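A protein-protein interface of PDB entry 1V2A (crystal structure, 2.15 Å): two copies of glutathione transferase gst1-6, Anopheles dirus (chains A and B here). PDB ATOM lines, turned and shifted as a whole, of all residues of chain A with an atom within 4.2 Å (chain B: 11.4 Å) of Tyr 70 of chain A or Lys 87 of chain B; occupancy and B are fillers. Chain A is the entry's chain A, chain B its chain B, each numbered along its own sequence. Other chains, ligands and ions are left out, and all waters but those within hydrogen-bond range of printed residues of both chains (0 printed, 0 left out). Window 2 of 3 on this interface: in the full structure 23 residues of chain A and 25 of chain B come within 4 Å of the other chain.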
ATOM      1  N   LEU A  54     -29.144 -20.694  -5.353  1.00  0.00           N
ATOM      2  CA  LEU A  54     -28.285 -19.595  -5.757  1.00  0.00           C
ATOM      3  C   LEU A  54     -26.862 -20.057  -5.995  1.00  0.00           C
ATOM      4  O   LEU A  54     -26.358 -20.922  -5.279  1.00  0.00           O
ATOM      5  CB  LEU A  54     -28.269 -18.519  -4.676  1.00  0.00           C
ATOM      6  CG  LEU A  54     -27.317 -17.346  -4.924  1.00  0.00           C
ATOM      7  CD1 LEU A  54     -27.859 -16.489  -6.050  1.00  0.00           C
ATOM      8  CD2 LEU A  54     -27.166 -16.522  -3.656  1.00  0.00           C
ATOM      9  N   ASP A  56     -23.370 -18.002  -6.522  1.00  0.00           N
ATOM     10  CA  ASP A  56     -22.704 -16.708  -6.568  1.00  0.00           C
ATOM     11  C   ASP A  56     -21.188 -16.807  -6.449  1.00  0.00           C
ATOM     12  O   ASP A  56     -20.660 -17.270  -5.442  1.00  0.00           O
ATOM     13  CB  ASP A  56     -23.275 -15.820  -5.464  1.00  0.00           C
ATOM     14  CG  ASP A  56     -22.545 -14.508  -5.330  1.00  0.00           C
ATOM     15  OD1 ASP A  56     -22.174 -13.918  -6.365  1.00  0.00           O
ATOM     16  OD2 ASP A  56     -22.352 -14.062  -4.181  1.00  0.00           O
ATOM     17  N   HIS A  59     -20.074 -20.020  -5.394  1.00  0.00           N
ATOM     18  CA  HIS A  59     -20.558 -20.502  -4.098  1.00  0.00           C
ATOM     19  C   HIS A  59     -22.047 -20.834  -4.174  1.00  0.00           C
ATOM     20  O   HIS A  59     -22.861 -19.978  -4.524  1.00  0.00           O
ATOM     21  CB  HIS A  59     -20.310 -19.441  -3.022  1.00  0.00           C
ATOM     22  CG  HIS A  59     -20.829 -19.814  -1.667  1.00  0.00           C
ATOM     23  ND1 HIS A  59     -20.440 -20.962  -1.008  1.00  0.00           N
ATOM     24  CD2 HIS A  59     -21.698 -19.183  -0.843  1.00  0.00           C
ATOM     25  CE1 HIS A  59     -21.049 -21.020   0.163  1.00  0.00           C
ATOM     26  NE2 HIS A  59     -21.817 -19.953   0.288  1.00  0.00           N
ATOM     27  N   ALA A  66     -31.817 -19.465   3.462  1.00  0.00           N
ATOM     28  CA  ALA A  66     -30.358 -19.380   3.472  1.00  0.00           C
ATOM     29  C   ALA A  66     -29.880 -18.468   2.349  1.00  0.00           C
ATOM     30  O   ALA A  66     -28.834 -17.840   2.448  1.00  0.00           O
ATOM     31  CB  ALA A  66     -29.753 -20.762   3.321  1.00  0.00           C
ATOM     32  N   ILE A  67     -30.651 -18.411   1.271  1.00  0.00           N
ATOM     33  CA  ILE A  67     -30.331 -17.553   0.135  1.00  0.00           C
ATOM     34  C   ILE A  67     -30.500 -16.092   0.564  1.00  0.00           C
ATOM     35  O   ILE A  67     -29.620 -15.258   0.373  1.00  0.00           O
ATOM     36  CB  ILE A  67     -31.299 -17.810  -1.043  1.00  0.00           C
ATOM     37  CG1 ILE A  67     -31.085 -19.215  -1.602  1.00  0.00           C
ATOM     38  CG2 ILE A  67     -31.110 -16.756  -2.109  1.00  0.00           C
ATOM     39  CD1 ILE A  67     -32.033 -19.561  -2.740  1.00  0.00           C
ATOM     40  N   VAL A  68     -31.649 -15.803   1.151  1.00  0.00           N
ATOM     41  CA  VAL A  68     -31.972 -14.461   1.601  1.00  0.00           C
ATOM     42  C   VAL A  68     -30.974 -13.888   2.600  1.00  0.00           C
ATOM     43  O   VAL A  68     -30.526 -12.742   2.452  1.00  0.00           O
ATOM     44  CB  VAL A  68     -33.394 -14.442   2.206  1.00  0.00           C
ATOM     45  CG1 VAL A  68     -33.606 -13.181   3.049  1.00  0.00           C
ATOM     46  CG2 VAL A  68     -34.413 -14.519   1.066  1.00  0.00           C
ATOM     47  N   LEU A  69     -30.624 -14.679   3.615  1.00  0.00           N
ATOM     48  CA  LEU A  69     -29.677 -14.225   4.628  1.00  0.00           C
ATOM     49  C   LEU A  69     -28.279 -14.007   4.045  1.00  0.00           C
ATOM     50  O   LEU A  69     -27.562 -13.071   4.430  1.00  0.00           O
ATOM     51  CB  LEU A  69     -29.631 -15.218   5.791  1.00  0.00           C
ATOM     52  CG  LEU A  69     -30.899 -15.266   6.653  1.00  0.00           C
ATOM     53  CD1 LEU A  69     -30.662 -16.157   7.854  1.00  0.00           C
ATOM     54  CD2 LEU A  69     -31.268 -13.869   7.126  1.00  0.00           C
ATOM     55  N   TYR A  70     -27.901 -14.861   3.103  1.00  0.00           N
ATOM     56  CA  TYR A  70     -26.598 -14.750   2.461  1.00  0.00           C
ATOM     57  C   TYR A  70     -26.528 -13.442   1.662  1.00  0.00           C
ATOM     58  O   TYR A  70     -25.534 -12.712   1.706  1.00  0.00           O
ATOM     59  CB  TYR A  70     -26.389 -15.939   1.524  1.00  0.00           C
ATOM     60  CG  TYR A  70     -25.201 -15.789   0.612  1.00  0.00           C
ATOM     61  CD1 TYR A  70     -23.923 -16.146   1.037  1.00  0.00           C
ATOM     62  CD2 TYR A  70     -25.350 -15.276  -0.675  1.00  0.00           C
ATOM     63  CE1 TYR A  70     -22.824 -16.001   0.204  1.00  0.00           C
ATOM     64  CE2 TYR A  70     -24.256 -15.124  -1.517  1.00  0.00           C
ATOM     65  CZ  TYR A  70     -22.998 -15.491  -1.072  1.00  0.00           C
ATOM     66  OH  TYR A  70     -21.910 -15.370  -1.905  1.00  0.00           O
ATOM     67  N   LEU A  71     -27.599 -13.161   0.927  1.00  0.00           N
ATOM     68  CA  LEU A  71     -27.665 -11.962   0.117  1.00  0.00           C
ATOM     69  C   LEU A  71     -27.530 -10.704   0.963  1.00  0.00           C
ATOM     70  O   LEU A  71     -26.725  -9.834   0.647  1.00  0.00           O
ATOM     71  CB  LEU A  71     -28.965 -11.944  -0.681  1.00  0.00           C
ATOM     72  CG  LEU A  71     -28.987 -13.010  -1.783  1.00  0.00           C
ATOM     73  CD1 LEU A  71     -30.345 -13.035  -2.455  1.00  0.00           C
ATOM     74  CD2 LEU A  71     -27.884 -12.721  -2.811  1.00  0.00           C
ATOM     75  N   VAL A  72     -28.305 -10.621   2.040  1.00  0.00           N
ATOM     76  CA  VAL A  72     -28.261  -9.469   2.936  1.00  0.00           C
ATOM     77  C   VAL A  72     -26.868  -9.259   3.525  1.00  0.00           C
ATOM     78  O   VAL A  72     -26.344  -8.148   3.515  1.00  0.00           O
ATOM     79  CB  VAL A  72     -29.267  -9.619   4.099  1.00  0.00           C
ATOM     80  CG1 VAL A  72     -29.000  -8.569   5.149  1.00  0.00           C
ATOM     81  CG2 VAL A  72     -30.680  -9.470   3.590  1.00  0.00           C
ATOM     82  N   GLU A  73     -26.268 -10.324   4.046  1.00  0.00           N
ATOM     83  CA  GLU A  73     -24.942 -10.214   4.637  1.00  0.00           C
ATOM     84  C   GLU A  73     -23.924  -9.801   3.589  1.00  0.00           C
ATOM     85  O   GLU A  73     -23.079  -8.937   3.826  1.00  0.00           O
ATOM     86  CB  GLU A  73     -24.509 -11.551   5.252  1.00  0.00           C
ATOM     87  CG  GLU A  73     -25.416 -12.069   6.359  1.00  0.00           C
ATOM     88  CD  GLU A  73     -24.832 -13.279   7.083  1.00  0.00           C
ATOM     89  OE1 GLU A  73     -24.553 -14.305   6.418  1.00  0.00           O
ATOM     90  OE2 GLU A  73     -24.651 -13.198   8.322  1.00  0.00           O
ATOM     91  N   THR A  74     -24.033 -10.415   2.419  1.00  0.00           N
ATOM     92  CA  THR A  74     -23.110 -10.181   1.320  1.00  0.00           C
ATOM     93  C   THR A  74     -23.324  -8.941   0.450  1.00  0.00           C
ATOM     94  O   THR A  74     -22.367  -8.435  -0.133  1.00  0.00           O
ATOM     95  CB  THR A  74     -23.092 -11.416   0.407  1.00  0.00           C
ATOM     96  OG1 THR A  74     -22.825 -12.577   1.206  1.00  0.00           O
ATOM     97  CG2 THR A  74     -22.025 -11.287  -0.675  1.00  0.00           C
ATOM     98  N   ASP B  79     -16.672 -17.847  17.528  1.00  0.00           N
ATOM     99  CA  ASP B  79     -17.691 -17.874  16.492  1.00  0.00           C
ATOM    100  C   ASP B  79     -17.518 -19.141  15.648  1.00  0.00           C
ATOM    101  O   ASP B  79     -18.050 -19.244  14.546  1.00  0.00           O
ATOM    102  CB  ASP B  79     -17.587 -16.625  15.616  1.00  0.00           C
ATOM    103  CG  ASP B  79     -18.192 -15.398  16.275  1.00  0.00           C
ATOM    104  OD1 ASP B  79     -19.426 -15.378  16.471  1.00  0.00           O
ATOM    105  OD2 ASP B  79     -17.438 -14.455  16.605  1.00  0.00           O
ATOM    106  N   TYR B  82     -20.630 -21.047  15.021  1.00  0.00           N
ATOM    107  CA  TYR B  82     -21.454 -20.332  14.062  1.00  0.00           C
ATOM    108  C   TYR B  82     -20.600 -19.275  13.342  1.00  0.00           C
ATOM    109  O   TYR B  82     -20.724 -18.074  13.583  1.00  0.00           O
ATOM    110  CB  TYR B  82     -22.648 -19.686  14.766  1.00  0.00           C
ATOM    111  CG  TYR B  82     -23.733 -19.233  13.817  1.00  0.00           C
ATOM    112  CD1 TYR B  82     -24.348 -20.138  12.946  1.00  0.00           C
ATOM    113  CD2 TYR B  82     -24.139 -17.900  13.775  1.00  0.00           C
ATOM    114  CE1 TYR B  82     -25.339 -19.722  12.055  1.00  0.00           C
ATOM    115  CE2 TYR B  82     -25.128 -17.477  12.892  1.00  0.00           C
ATOM    116  CZ  TYR B  82     -25.725 -18.390  12.033  1.00  0.00           C
ATOM    117  OH  TYR B  82     -26.708 -17.961  11.159  1.00  0.00           O
ATOM    118  N   PRO B  83     -19.716 -19.725  12.439  1.00  0.00           N
ATOM    119  CA  PRO B  83     -18.815 -18.878  11.656  1.00  0.00           C
ATOM    120  C   PRO B  83     -19.444 -17.638  11.007  1.00  0.00           C
ATOM    121  O   PRO B  83     -20.545 -17.687  10.458  1.00  0.00           O
ATOM    122  CB  PRO B  83     -18.253 -19.850  10.623  1.00  0.00           C
ATOM    123  CG  PRO B  83     -18.193 -21.129  11.384  1.00  0.00           C
ATOM    124  CD  PRO B  83     -19.521 -21.147  12.100  1.00  0.00           C
ATOM    125  N   LYS B  84     -18.707 -16.532  11.064  1.00  0.00           N
ATOM    126  CA  LYS B  84     -19.149 -15.265  10.504  1.00  0.00           C
ATOM    127  C   LYS B  84     -18.992 -15.163   8.990  1.00  0.00           C
ATOM    128  O   LYS B  84     -19.698 -14.386   8.343  1.00  0.00           O
ATOM    129  CB  LYS B  84     -18.391 -14.119  11.177  1.00  0.00           C
ATOM    130  CG  LYS B  84     -18.771 -13.941  12.632  1.00  0.00           C
ATOM    131  CD  LYS B  84     -17.966 -12.843  13.288  1.00  0.00           C
ATOM    132  CE  LYS B  84     -18.619 -12.420  14.582  1.00  0.00           C
ATOM    133  NZ  LYS B  84     -20.017 -11.974  14.332  1.00  0.00           N
ATOM    134  N   ASP B  85     -18.068 -15.935   8.421  1.00  0.00           N
ATOM    135  CA  ASP B  85     -17.862 -15.898   6.978  1.00  0.00           C
ATOM    136  C   ASP B  85     -19.102 -16.390   6.240  1.00  0.00           C
ATOM    137  O   ASP B  85     -19.446 -17.568   6.302  1.00  0.00           O
ATOM    138  CB  ASP B  85     -16.666 -16.745   6.573  1.00  0.00           C
ATOM    139  CG  ASP B  85     -16.695 -17.101   5.106  1.00  0.00           C
ATOM    140  OD1 ASP B  85     -16.930 -16.194   4.282  1.00  0.00           O
ATOM    141  OD2 ASP B  85     -16.488 -18.284   4.770  1.00  0.00           O
ATOM    142  N   PRO B  86     -19.785 -15.484   5.522  1.00  0.00           N
ATOM    143  CA  PRO B  86     -21.000 -15.795   4.761  1.00  0.00           C
ATOM    144  C   PRO B  86     -20.886 -17.024   3.872  1.00  0.00           C
ATOM    145  O   PRO B  86     -21.886 -17.667   3.574  1.00  0.00           O
ATOM    146  CB  PRO B  86     -21.239 -14.515   3.960  1.00  0.00           C
ATOM    147  CG  PRO B  86     -20.712 -13.458   4.878  1.00  0.00           C
ATOM    148  CD  PRO B  86     -19.410 -14.070   5.344  1.00  0.00           C
ATOM    149  N   LYS B  87     -19.670 -17.347   3.451  1.00  0.00           N
ATOM    150  CA  LYS B  87     -19.439 -18.508   2.596  1.00  0.00           C
ATOM    151  C   LYS B  87     -19.627 -19.793   3.402  1.00  0.00           C
ATOM    152  O   LYS B  87     -20.047 -20.823   2.870  1.00  0.00           O
ATOM    153  CB  LYS B  87     -18.020 -18.466   2.029  1.00  0.00           C
ATOM    154  CG  LYS B  87     -17.725 -17.263   1.135  1.00  0.00           C
ATOM    155  CD  LYS B  87     -18.210 -17.492  -0.291  1.00  0.00           C
ATOM    156  CE  LYS B  87     -17.987 -16.268  -1.178  1.00  0.00           C
ATOM    157  NZ  LYS B  87     -18.931 -15.145  -0.875  1.00  0.00           N
ATOM    158  N   VAL B  88     -19.302 -19.728   4.690  1.00  0.00           N
ATOM    159  CA  VAL B  88     -19.441 -20.879   5.575  1.00  0.00           C
ATOM    160  C   VAL B  88     -20.822 -20.891   6.213  1.00  0.00           C
ATOM    161  O   VAL B  88     -21.511 -21.911   6.210  1.00  0.00           O
ATOM    162  CB  VAL B  88     -18.390 -20.859   6.705  1.00  0.00           C
ATOM    163  CG1 VAL B  88     -18.583 -22.066   7.613  1.00  0.00           C
ATOM    164  CG2 VAL B  88     -16.987 -20.855   6.113  1.00  0.00           C
ATOM    165  N   ARG B  89     -21.215 -19.742   6.751  1.00  0.00           N
ATOM    166  CA  ARG B  89     -22.505 -19.588   7.411  1.00  0.00           C
ATOM    167  C   ARG B  89     -23.701 -19.972   6.546  1.00  0.00           C
ATOM    168  O   ARG B  89     -24.743 -20.356   7.071  1.00  0.00           O
ATOM    169  CB  ARG B  89     -22.672 -18.149   7.911  1.00  0.00           C
ATOM    170  CG  ARG B  89     -23.963 -17.933   8.679  1.00  0.00           C
ATOM    171  CD  ARG B  89     -23.953 -16.650   9.485  1.00  0.00           C
ATOM    172  NE  ARG B  89     -23.013 -16.713  10.598  1.00  0.00           N
ATOM    173  CZ  ARG B  89     -22.891 -15.771  11.528  1.00  0.00           C
ATOM    174  NH1 ARG B  89     -23.652 -14.690  11.481  1.00  0.00           N
ATOM    175  NH2 ARG B  89     -22.013 -15.914  12.511  1.00  0.00           N
ATOM    176  N   SER B  90     -23.564 -19.871   5.226  1.00  0.00           N
ATOM    177  CA  SER B  90     -24.666 -20.232   4.343  1.00  0.00           C
ATOM    178  C   SER B  90     -24.916 -21.733   4.410  1.00  0.00           C
ATOM    179  O   SER B  90     -26.061 -22.175   4.344  1.00  0.00           O
ATOM    180  CB  SER B  90     -24.396 -19.802   2.888  1.00  0.00           C
ATOM    181  OG  SER B  90     -23.245 -20.421   2.344  1.00  0.00           O
ATOM    182  N   VAL B  91     -23.855 -22.514   4.565  1.00  0.00           N
ATOM    183  CA  VAL B  91     -24.011 -23.966   4.641  1.00  0.00           C
ATOM    184  C   VAL B  91     -24.680 -24.348   5.961  1.00  0.00           C
ATOM    185  O   VAL B  91     -25.596 -25.167   5.989  1.00  0.00           O
ATOM    186  CB  VAL B  91     -22.658 -24.693   4.551  1.00  0.00           C
ATOM    187  CG1 VAL B  91     -22.893 -26.163   4.255  1.00  0.00           C
ATOM    188  CG2 VAL B  91     -21.789 -24.060   3.478  1.00  0.00           C
ATOM    189  N   VAL B  92     -24.215 -23.740   7.049  1.00  0.00           N
ATOM    190  CA  VAL B  92     -24.768 -23.999   8.370  1.00  0.00           C
ATOM    191  C   VAL B  92     -26.246 -23.652   8.324  1.00  0.00           C
ATOM    192  O   VAL B  92     -27.099 -24.476   8.664  1.00  0.00           O
ATOM    193  CB  VAL B  92     -24.061 -23.136   9.449  1.00  0.00           C
ATOM    194  CG1 VAL B  92     -24.606 -23.464  10.827  1.00  0.00           C
ATOM    195  CG2 VAL B  92     -22.557 -23.396   9.419  1.00  0.00           C
ATOM    196  N   ASN B  93     -26.553 -22.436   7.883  1.00  0.00           N
ATOM    197  CA  ASN B  93     -27.946 -22.012   7.789  1.00  0.00           C
ATOM    198  C   ASN B  93     -28.765 -22.970   6.953  1.00  0.00           C
ATOM    199  O   ASN B  93     -29.867 -23.354   7.348  1.00  0.00           O
ATOM    200  CB  ASN B  93     -28.058 -20.613   7.192  1.00  0.00           C
ATOM    201  CG  ASN B  93     -27.811 -19.534   8.214  1.00  0.00           C
ATOM    202  OD1 ASN B  93     -27.783 -19.801   9.415  1.00  0.00           O
ATOM    203  ND2 ASN B  93     -27.643 -18.309   7.749  1.00  0.00           N
ATOM    204  N   GLN B  94     -28.233 -23.358   5.796  1.00  0.00           N
ATOM    205  CA  GLN B  94     -28.948 -24.278   4.923  1.00  0.00           C
ATOM    206  C   GLN B  94     -29.185 -25.619   5.610  1.00  0.00           C
ATOM    207  O   GLN B  94     -30.291 -26.160   5.546  1.00  0.00           O
ATOM    208  CB  GLN B  94     -28.188 -24.483   3.616  1.00  0.00           C
ATOM    209  CG  GLN B  94     -28.840 -25.496   2.684  1.00  0.00           C
ATOM    210  CD  GLN B  94     -28.387 -26.916   2.958  1.00  0.00           C
ATOM    211  OE1 GLN B  94     -29.197 -27.802   3.243  1.00  0.00           O
ATOM    212  NE2 GLN B  94     -27.076 -27.141   2.872  1.00  0.00           N
ATOM    213  N   ARG B  95     -28.157 -26.148   6.275  1.00  0.00           N
ATOM    214  CA  ARG B  95     -28.291 -27.426   6.964  1.00  0.00           C
ATOM    215  C   ARG B  95     -29.319 -27.326   8.097  1.00  0.00           C
ATOM    216  O   ARG B  95     -29.975 -28.317   8.439  1.00  0.00           O
ATOM    217  CB  ARG B  95     -26.954 -27.887   7.554  1.00  0.00           C
ATOM    218  CG  ARG B  95     -25.750 -27.885   6.614  1.00  0.00           C
ATOM    219  CD  ARG B  95     -25.867 -28.827   5.430  1.00  0.00           C
ATOM    220  NE  ARG B  95     -24.553 -29.323   5.028  1.00  0.00           N
ATOM    221  CZ  ARG B  95     -24.203 -29.630   3.781  1.00  0.00           C
ATOM    222  NH1 ARG B  95     -25.068 -29.486   2.785  1.00  0.00           N
ATOM    223  NH2 ARG B  95     -22.988 -30.097   3.532  1.00  0.00           N
ATOM    224  N   PHE B  97     -32.037 -25.392   8.036  1.00  0.00           N
ATOM    225  CA  PHE B  97     -33.359 -25.396   7.426  1.00  0.00           C
ATOM    226  C   PHE B  97     -33.660 -26.760   6.838  1.00  0.00           C
ATOM    227  O   PHE B  97     -34.816 -27.123   6.616  1.00  0.00           O
ATOM    228  CB  PHE B  97     -33.486 -24.282   6.380  1.00  0.00           C
ATOM    229  CG  PHE B  97     -33.687 -22.920   6.994  1.00  0.00           C
ATOM    230  CD1 PHE B  97     -32.604 -22.091   7.256  1.00  0.00           C
ATOM    231  CD2 PHE B  97     -34.957 -22.500   7.375  1.00  0.00           C
ATOM    232  CE1 PHE B  97     -32.777 -20.855   7.894  1.00  0.00           C
ATOM    233  CE2 PHE B  97     -35.146 -21.274   8.016  1.00  0.00           C
ATOM    234  CZ  PHE B  97     -34.051 -20.447   8.276  1.00  0.00           C
ATOM    235  N   GLU B 141     -18.789 -35.295   2.433  1.00  0.00           N
ATOM    236  CA  GLU B 141     -18.065 -34.204   1.805  1.00  0.00           C
ATOM    237  C   GLU B 141     -17.198 -33.522   2.868  1.00  0.00           C
ATOM    238  O   GLU B 141     -16.171 -32.916   2.557  1.00  0.00           O
ATOM    239  CB  GLU B 141     -19.044 -33.220   1.163  1.00  0.00           C
ATOM    240  CG  GLU B 141     -20.120 -32.693   2.089  1.00  0.00           C
ATOM    241  CD  GLU B 141     -21.199 -31.917   1.345  1.00  0.00           C
ATOM    242  OE1 GLU B 141     -20.858 -30.984   0.589  1.00  0.00           O
ATOM    243  OE2 GLU B 141     -22.394 -32.237   1.521  1.00  0.00           O
ATOM    244  N   ARG B 142     -17.620 -33.634   4.126  1.00  0.00           N
ATOM    245  CA  ARG B 142     -16.867 -33.082   5.248  1.00  0.00           C
ATOM    246  C   ARG B 142     -17.100 -33.985   6.454  1.00  0.00           C
ATOM    247  O   ARG B 142     -18.046 -34.775   6.471  1.00  0.00           O
ATOM    248  CB  ARG B 142     -17.310 -31.654   5.600  1.00  0.00           C
ATOM    249  CG  ARG B 142     -17.383 -30.684   4.441  1.00  0.00           C
ATOM    250  CD  ARG B 142     -17.319 -29.245   4.942  1.00  0.00           C
ATOM    251  NE  ARG B 142     -17.707 -28.284   3.914  1.00  0.00           N
ATOM    252  CZ  ARG B 142     -18.956 -28.111   3.480  1.00  0.00           C
ATOM    253  NH1 ARG B 142     -19.956 -28.834   3.983  1.00  0.00           N
ATOM    254  NH2 ARG B 142     -19.210 -27.206   2.541  1.00  0.00           N
ATOM    255  N   ALA B 145     -21.399 -31.745   9.856  1.00  0.00           N
ATOM    256  CA  ALA B 145     -22.629 -31.357   9.172  1.00  0.00           C
ATOM    257  C   ALA B 145     -22.542 -30.223   8.156  1.00  0.00           C
ATOM    258  O   ALA B 145     -23.054 -30.358   7.040  1.00  0.00           O
ATOM    259  CB  ALA B 145     -23.715 -31.042  10.198  1.00  0.00           C
ATOM    260  N   ALA B 146     -21.911 -29.111   8.533  1.00  0.00           N
ATOM    261  CA  ALA B 146     -21.807 -27.963   7.640  1.00  0.00           C
ATOM    262  C   ALA B 146     -20.411 -27.357   7.482  1.00  0.00           C
ATOM    263  O   ALA B 146     -20.261 -26.297   6.876  1.00  0.00           O
ATOM    264  CB  ALA B 146     -22.783 -26.883   8.091  1.00  0.00           C
ATOM    265  N   ALA B 147     -19.385 -28.000   8.020  1.00  0.00           N
ATOM    266  CA  ALA B 147     -18.050 -27.440   7.882  1.00  0.00           C
ATOM    267  C   ALA B 147     -16.973 -28.449   8.231  1.00  0.00           C
ATOM    268  O   ALA B 147     -17.257 -29.636   8.404  1.00  0.00           O
ATOM    269  CB  ALA B 147     -17.914 -26.196   8.770  1.00  0.00           C
ATOM    270  N   ASP B 148     -15.741 -27.959   8.325  1.00  0.00           N
ATOM    271  CA  ASP B 148     -14.580 -28.774   8.657  1.00  0.00           C
ATOM    272  C   ASP B 148     -14.419 -28.847  10.181  1.00  0.00           C
ATOM    273  O   ASP B 148     -13.375 -29.241  10.701  1.00  0.00           O
ATOM    274  CB  ASP B 148     -13.329 -28.167   8.012  1.00  0.00           C
ATOM    275  CG  ASP B 148     -12.922 -26.843   8.653  1.00  0.00           C
ATOM    276  OD1 ASP B 148     -13.806 -26.121   9.171  1.00  0.00           O
ATOM    277  OD2 ASP B 148     -11.716 -26.526   8.630  1.00  0.00           O
ATOM    278  N   HIS B 149     -15.465 -28.450  10.893  1.00  0.00           N
ATOM    279  CA  HIS B 149     -15.470 -28.490  12.348  1.00  0.00           C
ATOM    280  C   HIS B 149     -16.915 -28.397  12.844  1.00  0.00           C
ATOM    281  O   HIS B 149     -17.814 -28.016  12.100  1.00  0.00           O
ATOM    282  CB  HIS B 149     -14.634 -27.340  12.944  1.00  0.00           C
ATOM    283  CG  HIS B 149     -15.253 -25.990  12.778  1.00  0.00           C
ATOM    284  ND1 HIS B 149     -15.104 -25.235  11.634  1.00  0.00           N
ATOM    285  CD2 HIS B 149     -16.081 -25.286  13.587  1.00  0.00           C
ATOM    286  CE1 HIS B 149     -15.819 -24.129  11.743  1.00  0.00           C
ATOM    287  NE2 HIS B 149     -16.422 -24.135  12.918  1.00  0.00           N
ATOM    288  N   THR B 151     -20.376 -27.257  14.452  1.00  0.00           N
ATOM    289  CA  THR B 151     -21.119 -26.005  14.441  1.00  0.00           C
ATOM    290  C   THR B 151     -22.486 -26.303  15.050  1.00  0.00           C
ATOM    291  O   THR B 151     -22.760 -27.436  15.444  1.00  0.00           O
ATOM    292  CB  THR B 151     -21.314 -25.454  13.000  1.00  0.00           C
ATOM    293  OG1 THR B 151     -22.124 -26.353  12.231  1.00  0.00           O
ATOM    294  CG2 THR B 151     -19.973 -25.283  12.309  1.00  0.00           C
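No position is printed for both chains. Of the 8 pairs that touch across the chains among the printed residues, none has its exchanged pair printed and touching as well.
Printed residues of chain B that touch a printed residue of chain A: Pro 86, Lys 87, Arg 89, Ser 90, Asn 93 and Gln 94. Hydrophobic or aromatic side chains of chain B within 4 Å of the printed part of chain A: Pro 86. Hydrophobic or aromatic side chains of chain A that line the printed part of chain B: His 59, Ala 66, Leu 69 and Tyr 70. Among the printed residues, Asp or Glu carboxylates within 4 Å of a Lys or Arg side-chain nitrogen of the other chain: Glu 73 of chain A with Arg 89 of chain B.
Gln 94 of chain B touches Ala 66 of chain A (N to CB, 3.9 Å). ND2 of Asn 93 of chain B touches CD1 of Leu 69 of chain A, 3.7 Å away. Pro 86 of chain B touches Tyr 70 of chain A. Thr 74 of chain A touches Pro 86 of chain B.
OD1 of Asn 93 of chain B is in hydrogen-bond range of OH of Tyr 82 of chain B (2.8 Å). NH1 of Arg 95 of chain B sits close to NE2 of Gln 94 of chain B (3.1 Å). The backbone carbonyl oxygen of Lys 87 of chain B sits at hydrogen-bond distance from the side-chain hydroxyl of Ser 90 of chain B, at 3.3 Å. OD1 of Asp 85 of chain B sits close to N of Lys 87 of chain B (3.1 Å). The side-chain hydroxyl of Ser 90 of chain B is in hydrogen-bond range of the backbone carbonyl oxygen of Pro 86 of chain B (3.3 Å). The backbone carbonyl oxygen (O) of Pro 83 of chain B is in hydrogen-bond range of the guanidinium group (NE) of Arg 89 of chain B (2.7 Å).
OE2 of Glu 73 of chain A lies within salt-bridge range of NH1 of Arg 89 of chain B. A ring nitrogen (NE2) of His 59 of chain A lies close to the backbone carbonyl oxygen (O) of Lys 87 of chain B, 3.2 Å away. OH of Tyr 70 of chain A lies within hydrogen-bond range of NZ of Lys 87 of chain B. The side-chain hydroxyl of Ser 90 of chain B lies within hydrogen-bond range of a ring nitrogen (NE2) of His 59 of chain A (2.5 Å).
Of the printed residues of chain B, His 59 of chain A touches Lys 87 (2.9 Å) and Ser 90 (2.5 Å). Of chain B, only Gln 94 comes within 4 Å of Ala 66 of chain A. No residue of chain B comes within 4 Å of Val 68 of chain A. Of chain B, only Pro 86 and Lys 87 come within 4 Å of Tyr 70 of chain A. No residue of chain B comes within 4 Å of Leu 71 of chain A. Val 72 of chain A touches none of the printed residues of chain B. Of chain B, only Pro 86 (3.7 Å) comes within 4 Å of Thr 74 of chain A. Printed residues of chain A within 4 Å of Pro 86 of chain B: Tyr 70 and Thr 74. Of chain A, only His 59 and Tyr 70 come within 4 Å of Lys 87 of chain B. Ala 145 of chain B touches none of the printed residues of chain A. Ala 146 of chain B touches none of the printed residues of chain A. The nearest printed residue of chain A that does not touch Asn 93 of chain B is Ala 66 of chain A (4.2 Å).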
